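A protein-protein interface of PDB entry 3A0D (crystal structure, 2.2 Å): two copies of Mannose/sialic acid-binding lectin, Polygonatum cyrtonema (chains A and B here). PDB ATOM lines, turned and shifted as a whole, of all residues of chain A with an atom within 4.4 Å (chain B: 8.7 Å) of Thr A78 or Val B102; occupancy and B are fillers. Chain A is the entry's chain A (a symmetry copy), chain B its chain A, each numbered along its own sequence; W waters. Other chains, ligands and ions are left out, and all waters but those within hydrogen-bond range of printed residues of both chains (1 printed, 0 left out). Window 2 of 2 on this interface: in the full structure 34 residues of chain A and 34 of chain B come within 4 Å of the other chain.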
ATOM      1  N   ASN A  60      20.473  20.730  19.272  1.00  0.00           N
ATOM      2  CA  ASN A  60      20.575  21.147  20.666  1.00  0.00           C
ATOM      3  C   ASN A  60      21.067  19.975  21.520  1.00  0.00           C
ATOM      4  O   ASN A  60      21.178  20.085  22.740  1.00  0.00           O
ATOM      5  CB  ASN A  60      19.224  21.683  21.176  1.00  0.00           C
ATOM      6  CG  ASN A  60      18.250  20.583  21.540  1.00  0.00           C
ATOM      7  OD1 ASN A  60      18.274  19.493  20.967  1.00  0.00           O
ATOM      8  ND2 ASN A  60      17.369  20.873  22.491  1.00  0.00           N
ATOM      9  N   GLY A  61      21.368  18.853  20.863  1.00  0.00           N
ATOM     10  CA  GLY A  61      21.877  17.687  21.570  1.00  0.00           C
ATOM     11  C   GLY A  61      20.887  16.584  21.905  1.00  0.00           C
ATOM     12  O   GLY A  61      21.283  15.512  22.367  1.00  0.00           O
ATOM     13  N   ASN A  62      19.603  16.821  21.672  1.00  0.00           N
ATOM     14  CA  ASN A  62      18.601  15.809  21.986  1.00  0.00           C
ATOM     15  C   ASN A  62      18.524  14.735  20.901  1.00  0.00           C
ATOM     16  O   ASN A  62      18.433  15.045  19.711  1.00  0.00           O
ATOM     17  CB  ASN A  62      17.234  16.475  22.182  1.00  0.00           C
ATOM     18  CG  ASN A  62      16.226  15.555  22.846  1.00  0.00           C
ATOM     19  OD1 ASN A  62      16.590  14.715  23.669  1.00  0.00           O
ATOM     20  ND2 ASN A  62      14.949  15.725  22.508  1.00  0.00           N
ATOM     21  N   LEU A  63      18.585  13.472  21.320  1.00  0.00           N
ATOM     22  CA  LEU A  63      18.509  12.339  20.401  1.00  0.00           C
ATOM     23  C   LEU A  63      17.105  11.743  20.510  1.00  0.00           C
ATOM     24  O   LEU A  63      16.656  11.378  21.596  1.00  0.00           O
ATOM     25  CB  LEU A  63      19.564  11.286  20.769  1.00  0.00           C
ATOM     26  CG  LEU A  63      19.671  10.069  19.846  1.00  0.00           C
ATOM     27  CD1 LEU A  63      20.110  10.509  18.451  1.00  0.00           C
ATOM     28  CD2 LEU A  63      20.663   9.070  20.430  1.00  0.00           C
ATOM     29  N   THR A  76      16.534  10.950  24.521  1.00  0.00           N
ATOM     30  CA  THR A  76      17.507  11.056  25.604  1.00  0.00           C
ATOM     31  C   THR A  76      17.199  12.238  26.518  1.00  0.00           C
ATOM     32  O   THR A  76      17.702  12.314  27.639  1.00  0.00           O
ATOM     33  CB  THR A  76      18.938  11.232  25.055  1.00  0.00           C
ATOM     34  OG1 THR A  76      18.976  12.359  24.170  1.00  0.00           O
ATOM     35  CG2 THR A  76      19.389   9.981  24.309  1.00  0.00           C
ATOM     36  N   LYS A  77      16.371  13.157  26.034  1.00  0.00           N
ATOM     37  CA  LYS A  77      15.998  14.347  26.793  1.00  0.00           C
ATOM     38  C   LYS A  77      17.226  15.165  27.168  1.00  0.00           C
ATOM     39  O   LYS A  77      17.335  15.674  28.285  1.00  0.00           O
ATOM     40  CB  LYS A  77      15.227  13.964  28.061  1.00  0.00           C
ATOM     41  CG  LYS A  77      13.902  13.268  27.791  1.00  0.00           C
ATOM     42  CD  LYS A  77      13.118  13.037  29.078  1.00  0.00           C
ATOM     43  CE  LYS A  77      11.790  12.344  28.804  1.00  0.00           C
ATOM     44  NZ  LYS A  77      10.976  12.194  30.045  1.00  0.00           N
ATOM     45  N   THR A  78      18.157  15.284  26.230  1.00  0.00           N
ATOM     46  CA  THR A  78      19.366  16.056  26.469  1.00  0.00           C
ATOM     47  C   THR A  78      19.281  17.346  25.664  1.00  0.00           C
ATOM     48  O   THR A  78      19.916  17.496  24.618  1.00  0.00           O
ATOM     49  CB  THR A  78      20.621  15.245  26.080  1.00  0.00           C
ATOM     50  OG1 THR A  78      20.413  14.613  24.810  1.00  0.00           O
ATOM     51  CG2 THR A  78      20.907  14.174  27.132  1.00  0.00           C
ATOM     52  N   ASN A  79      18.467  18.270  26.164  1.00  0.00           N
ATOM     53  CA  ASN A  79      18.249  19.558  25.526  1.00  0.00           C
ATOM     54  C   ASN A  79      19.235  20.585  26.067  1.00  0.00           C
ATOM     55  O   ASN A  79      19.119  21.025  27.215  1.00  0.00           O
ATOM     56  CB  ASN A  79      16.813  20.018  25.782  1.00  0.00           C
ATOM     57  CG  ASN A  79      15.792  19.050  25.224  1.00  0.00           C
ATOM     58  OD1 ASN A  79      15.700  18.859  24.009  1.00  0.00           O
ATOM     59  ND2 ASN A  79      15.022  18.422  26.108  1.00  0.00           N
ATOM     60  N   GLY A  80      20.199  20.966  25.236  1.00  0.00           N
ATOM     61  CA  GLY A  80      21.198  21.926  25.667  1.00  0.00           C
ATOM     62  C   GLY A  80      21.290  23.152  24.785  1.00  0.00           C
ATOM     63  O   GLY A  80      20.306  23.572  24.180  1.00  0.00           O
ATOM     64  N   TYR A  85      25.820  18.964  17.114  1.00  0.00           N
ATOM     65  CA  TYR A  85      26.319  17.822  17.870  1.00  0.00           C
ATOM     66  C   TYR A  85      26.541  16.620  16.971  1.00  0.00           C
ATOM     67  O   TYR A  85      26.210  16.646  15.784  1.00  0.00           O
ATOM     68  CB  TYR A  85      25.327  17.456  18.978  1.00  0.00           C
ATOM     69  CG  TYR A  85      25.096  18.568  19.978  1.00  0.00           C
ATOM     70  CD1 TYR A  85      24.366  19.706  19.634  1.00  0.00           C
ATOM     71  CD2 TYR A  85      25.644  18.500  21.259  1.00  0.00           C
ATOM     72  CE1 TYR A  85      24.193  20.751  20.537  1.00  0.00           C
ATOM     73  CE2 TYR A  85      25.478  19.533  22.167  1.00  0.00           C
ATOM     74  CZ  TYR A  85      24.755  20.657  21.801  1.00  0.00           C
ATOM     75  OH  TYR A  85      24.620  21.694  22.695  1.00  0.00           O
ATOM     76  N   ILE A  97      27.156  10.885  22.478  1.00  0.00           N
ATOM     77  CA  ILE A  97      26.727  12.143  21.884  1.00  0.00           C
ATOM     78  C   ILE A  97      27.714  13.192  22.395  1.00  0.00           C
ATOM     79  O   ILE A  97      27.894  13.338  23.608  1.00  0.00           O
ATOM     80  CB  ILE A  97      25.309  12.559  22.340  1.00  0.00           C
ATOM     81  CG1 ILE A  97      24.269  11.564  21.818  1.00  0.00           C
ATOM     82  CG2 ILE A  97      24.992  13.964  21.827  1.00  0.00           C
ATOM     83  CD1 ILE A  97      22.847  11.894  22.240  1.00  0.00           C
ATOM     84  N   GLY A  99      29.228  17.353  22.010  1.00  0.00           N
ATOM     85  CA  GLY A  99      28.857  18.683  21.567  1.00  0.00           C
ATOM     86  C   GLY A  99      28.976  19.671  22.705  1.00  0.00           C
ATOM     87  O   GLY A  99      29.053  19.260  23.861  1.00  0.00           O
ATOM     88  N   LYS B  81      37.313  22.273  28.996  1.00  0.00           N
ATOM     89  CA  LYS B  81      37.030  21.461  30.166  1.00  0.00           C
ATOM     90  C   LYS B  81      37.534  20.032  29.987  1.00  0.00           C
ATOM     91  O   LYS B  81      37.467  19.466  28.895  1.00  0.00           O
ATOM     92  CB  LYS B  81      35.523  21.454  30.449  1.00  0.00           C
ATOM     93  CG  LYS B  81      35.147  20.819  31.780  1.00  0.00           C
ATOM     94  CD  LYS B  81      34.478  19.461  31.606  1.00  0.00           C
ATOM     95  CE  LYS B  81      33.071  19.595  31.038  1.00  0.00           C
ATOM     96  NZ  LYS B  81      32.402  18.267  30.881  1.00  0.00           N
ATOM     97  N   ASP B  83      37.345  16.278  30.011  1.00  0.00           N
ATOM     98  CA  ASP B  83      36.243  15.337  29.832  1.00  0.00           C
ATOM     99  C   ASP B  83      36.628  14.364  28.714  1.00  0.00           C
ATOM    100  O   ASP B  83      37.601  13.622  28.835  1.00  0.00           O
ATOM    101  CB  ASP B  83      34.975  16.111  29.451  1.00  0.00           C
ATOM    102  CG  ASP B  83      33.712  15.310  29.681  1.00  0.00           C
ATOM    103  OD1 ASP B  83      32.946  15.094  28.715  1.00  0.00           O
ATOM    104  OD2 ASP B  83      33.486  14.894  30.836  1.00  0.00           O
ATOM    105  N   HIS B  84      35.852  14.367  27.635  1.00  0.00           N
ATOM    106  CA  HIS B  84      36.124  13.528  26.471  1.00  0.00           C
ATOM    107  C   HIS B  84      35.574  14.211  25.228  1.00  0.00           C
ATOM    108  O   HIS B  84      34.513  14.838  25.265  1.00  0.00           O
ATOM    109  CB  HIS B  84      35.502  12.136  26.623  1.00  0.00           C
ATOM    110  CG  HIS B  84      36.284  11.224  27.515  1.00  0.00           C
ATOM    111  ND1 HIS B  84      36.030  11.105  28.864  1.00  0.00           N
ATOM    112  CD2 HIS B  84      37.353  10.432  27.262  1.00  0.00           C
ATOM    113  CE1 HIS B  84      36.910  10.281  29.404  1.00  0.00           C
ATOM    114  NE2 HIS B  84      37.726   9.859  28.454  1.00  0.00           N
ATOM    115  N   TYR B  98      34.004  17.817  18.467  1.00  0.00           N
ATOM    116  CA  TYR B  98      32.821  18.026  19.303  1.00  0.00           C
ATOM    117  C   TYR B  98      33.108  17.602  20.733  1.00  0.00           C
ATOM    118  O   TYR B  98      33.890  16.686  20.970  1.00  0.00           O
ATOM    119  CB  TYR B  98      31.630  17.198  18.819  1.00  0.00           C
ATOM    120  CG  TYR B  98      31.059  17.576  17.480  1.00  0.00           C
ATOM    121  CD1 TYR B  98      31.511  16.961  16.311  1.00  0.00           C
ATOM    122  CD2 TYR B  98      30.011  18.490  17.383  1.00  0.00           C
ATOM    123  CE1 TYR B  98      30.923  17.240  15.082  1.00  0.00           C
ATOM    124  CE2 TYR B  98      29.418  18.776  16.157  1.00  0.00           C
ATOM    125  CZ  TYR B  98      29.879  18.145  15.012  1.00  0.00           C
ATOM    126  OH  TYR B  98      29.291  18.416  13.799  1.00  0.00           O
ATOM    127  N   GLY B  99      32.442  18.250  21.680  1.00  0.00           N
ATOM    128  CA  GLY B  99      32.635  17.910  23.076  1.00  0.00           C
ATOM    129  C   GLY B  99      32.138  19.026  23.966  1.00  0.00           C
ATOM    130  O   GLY B  99      31.933  20.140  23.486  1.00  0.00           O
ATOM    131  N   PRO B 100      31.962  18.775  25.273  1.00  0.00           N
ATOM    132  CA  PRO B 100      32.215  17.496  25.940  1.00  0.00           C
ATOM    133  C   PRO B 100      31.094  16.474  25.757  1.00  0.00           C
ATOM    134  O   PRO B 100      30.236  16.619  24.883  1.00  0.00           O
ATOM    135  CB  PRO B 100      32.379  17.909  27.394  1.00  0.00           C
ATOM    136  CG  PRO B 100      31.353  18.988  27.516  1.00  0.00           C
ATOM    137  CD  PRO B 100      31.562  19.802  26.250  1.00  0.00           C
ATOM    138  N   VAL B 101      31.110  15.446  26.596  1.00  0.00           N
ATOM    139  CA  VAL B 101      30.105  14.392  26.538  1.00  0.00           C
ATOM    140  C   VAL B 101      28.732  14.892  26.973  1.00  0.00           C
ATOM    141  O   VAL B 101      28.590  15.528  28.017  1.00  0.00           O
ATOM    142  CB  VAL B 101      30.490  13.194  27.433  1.00  0.00           C
ATOM    143  CG1 VAL B 101      29.367  12.171  27.441  1.00  0.00           C
ATOM    144  CG2 VAL B 101      31.775  12.555  26.930  1.00  0.00           C
ATOM    145  N   VAL B 102      27.726  14.602  26.156  1.00  0.00           N
ATOM    146  CA  VAL B 102      26.356  14.995  26.443  1.00  0.00           C
ATOM    147  C   VAL B 102      25.563  13.796  26.955  1.00  0.00           C
ATOM    148  O   VAL B 102      24.729  13.923  27.850  1.00  0.00           O
ATOM    149  CB  VAL B 102      25.661  15.540  25.171  1.00  0.00           C
ATOM    150  CG1 VAL B 102      24.147  15.576  25.368  1.00  0.00           C
ATOM    151  CG2 VAL B 102      26.183  16.933  24.851  1.00  0.00           C
ATOM    152  N   TRP B 103      25.846  12.627  26.388  1.00  0.00           N
ATOM    153  CA  TRP B 103      25.139  11.402  26.740  1.00  0.00           C
ATOM    154  C   TRP B 103      25.938  10.208  26.235  1.00  0.00           C
ATOM    155  O   TRP B 103      26.673  10.321  25.257  1.00  0.00           O
ATOM    156  CB  TRP B 103      23.762  11.416  26.066  1.00  0.00           C
ATOM    157  CG  TRP B 103      22.922  10.193  26.274  1.00  0.00           C
ATOM    158  CD1 TRP B 103      22.092   9.935  27.330  1.00  0.00           C
ATOM    159  CD2 TRP B 103      22.798   9.077  25.385  1.00  0.00           C
ATOM    160  NE1 TRP B 103      21.454   8.731  27.149  1.00  0.00           N
ATOM    161  CE2 TRP B 103      21.870   8.182  25.962  1.00  0.00           C
ATOM    162  CE3 TRP B 103      23.379   8.746  24.153  1.00  0.00           C
ATOM    163  CZ2 TRP B 103      21.510   6.976  25.350  1.00  0.00           C
ATOM    164  CZ3 TRP B 103      23.018   7.544  23.542  1.00  0.00           C
ATOM    165  CH2 TRP B 103      22.094   6.677  24.144  1.00  0.00           C
ATOM    166  N   ALA B 104      25.787   9.065  26.896  1.00  0.00           N
ATOM    167  CA  ALA B 104      26.484   7.846  26.494  1.00  0.00           C
ATOM    168  C   ALA B 104      25.661   6.623  26.888  1.00  0.00           C
ATOM    169  O   ALA B 104      24.962   6.636  27.897  1.00  0.00           O
ATOM    170  CB  ALA B 104      27.857   7.784  27.147  1.00  0.00           C
ATOM    171  N   THR B 105      25.744   5.568  26.084  1.00  0.00           N
ATOM    172  CA  THR B 105      25.010   4.337  26.357  1.00  0.00           C
ATOM    173  C   THR B 105      25.712   3.549  27.451  1.00  0.00           C
ATOM    174  O   THR B 105      25.083   2.803  28.197  1.00  0.00           O
ATOM    175  CB  THR B 105      24.957   3.426  25.124  1.00  0.00           C
ATOM    176  OG1 THR B 105      26.296   3.125  24.711  1.00  0.00           O
ATOM    177  CG2 THR B 105      24.195   4.095  23.989  1.00  0.00           C
HETATM  178  O   HOH W   1      26.478  18.627  13.338  1.00  0.00           O
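Of the 11 printed residues of chain B, 6 touch a printed residue of chain A.
Hydrophobic or aromatic side chains of chain B that line the printed part of chain A: Tyr B98, Pro B100, Val B102 and Trp B103.
Printed residues of chain A that touch a printed residue of chain B: Thr A76, Thr A78, Tyr A85, Ile A97 and Gly A99.
Hydrophobic or aromatic side chains of chain A that line the printed part of chain B: Tyr A85 and Ile A97.
Water W1 bridges OH of Tyr B98 (2.9 Å) and O of Tyr A85 (3.2 Å).
N of Gly A99 lies within hydrogen-bond range of O of Pro B100, at 3.1 Å.
The backbone NH of Val B102 sits at hydrogen-bond distance from the backbone carbonyl oxygen of Ile A97, at 2.8 Å.
N of Ile A97 is in hydrogen-bond range of O of Trp B103.
O of Gly A99 sits close to O of Gly B99.
Printed residues of chain B within 4 Å of Thr A78: Val B102.
Of the printed residues of chain A, Val B102 touches Thr A78, Tyr A85, Ile A97 and Gly A99.
No residue of chain B comes within 4 Å of Asn A79.
Printed residues of chain A within 4 Å of Val B101: Ile A97 (3.8 Å).
Of the printed residues of chain A, Tyr B98 touches Tyr A85 (3.7 Å) and Gly A99 (3.997 Å).
Of the printed residues of chain A, Trp B103 touches Thr A76 (3.5 Å) and Ile A97 (2.9 Å).
Of the printed residues of chain B, Tyr A85 touches Tyr B98 (3.7 Å) and Val B102 (3.8 Å).
Printed residues of chain A within 4 Å of Gly B99: Gly A99 (3.0 Å).
The nearest printed residue of chain A that does not touch Val B101 is Gly A99 (5.1 Å).
Gly B99 touches its own counterpart, Gly A99.
Position printed for both chains: 99.
Among the printed residues, merely in contact across the chains: Thr A76 with Trp B103, Thr A78 with Val B102, Tyr A85 with Tyr B98, Ile A97 with Val B101, Tyr A85 with Val B102, Gly A99 with Val B102 and Gly A99 with Tyr B98.
OD1 of Asp B83 lies within hydrogen-bond range of N of Val B101.
OG1 of Thr A78 sits at hydrogen-bond distance from O of Gly A61, 2.7 Å away.
The side-chain amide oxygen (OD1) of Asn A62 sits at hydrogen-bond distance from the side-chain hydroxyl (OG1) of Thr A76 (3.4 Å).
O of Thr A78 sits at hydrogen-bond distance from N of Asn A62, 3.0 Å away.
The backbone NH (N) of Thr A76 sits at hydrogen-bond distance from the backbone carbonyl oxygen (O) of Leu A63.
The side-chain hydroxyl of Thr A76 is in hydrogen-bond range of the side-chain hydroxyl of Thr A78.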
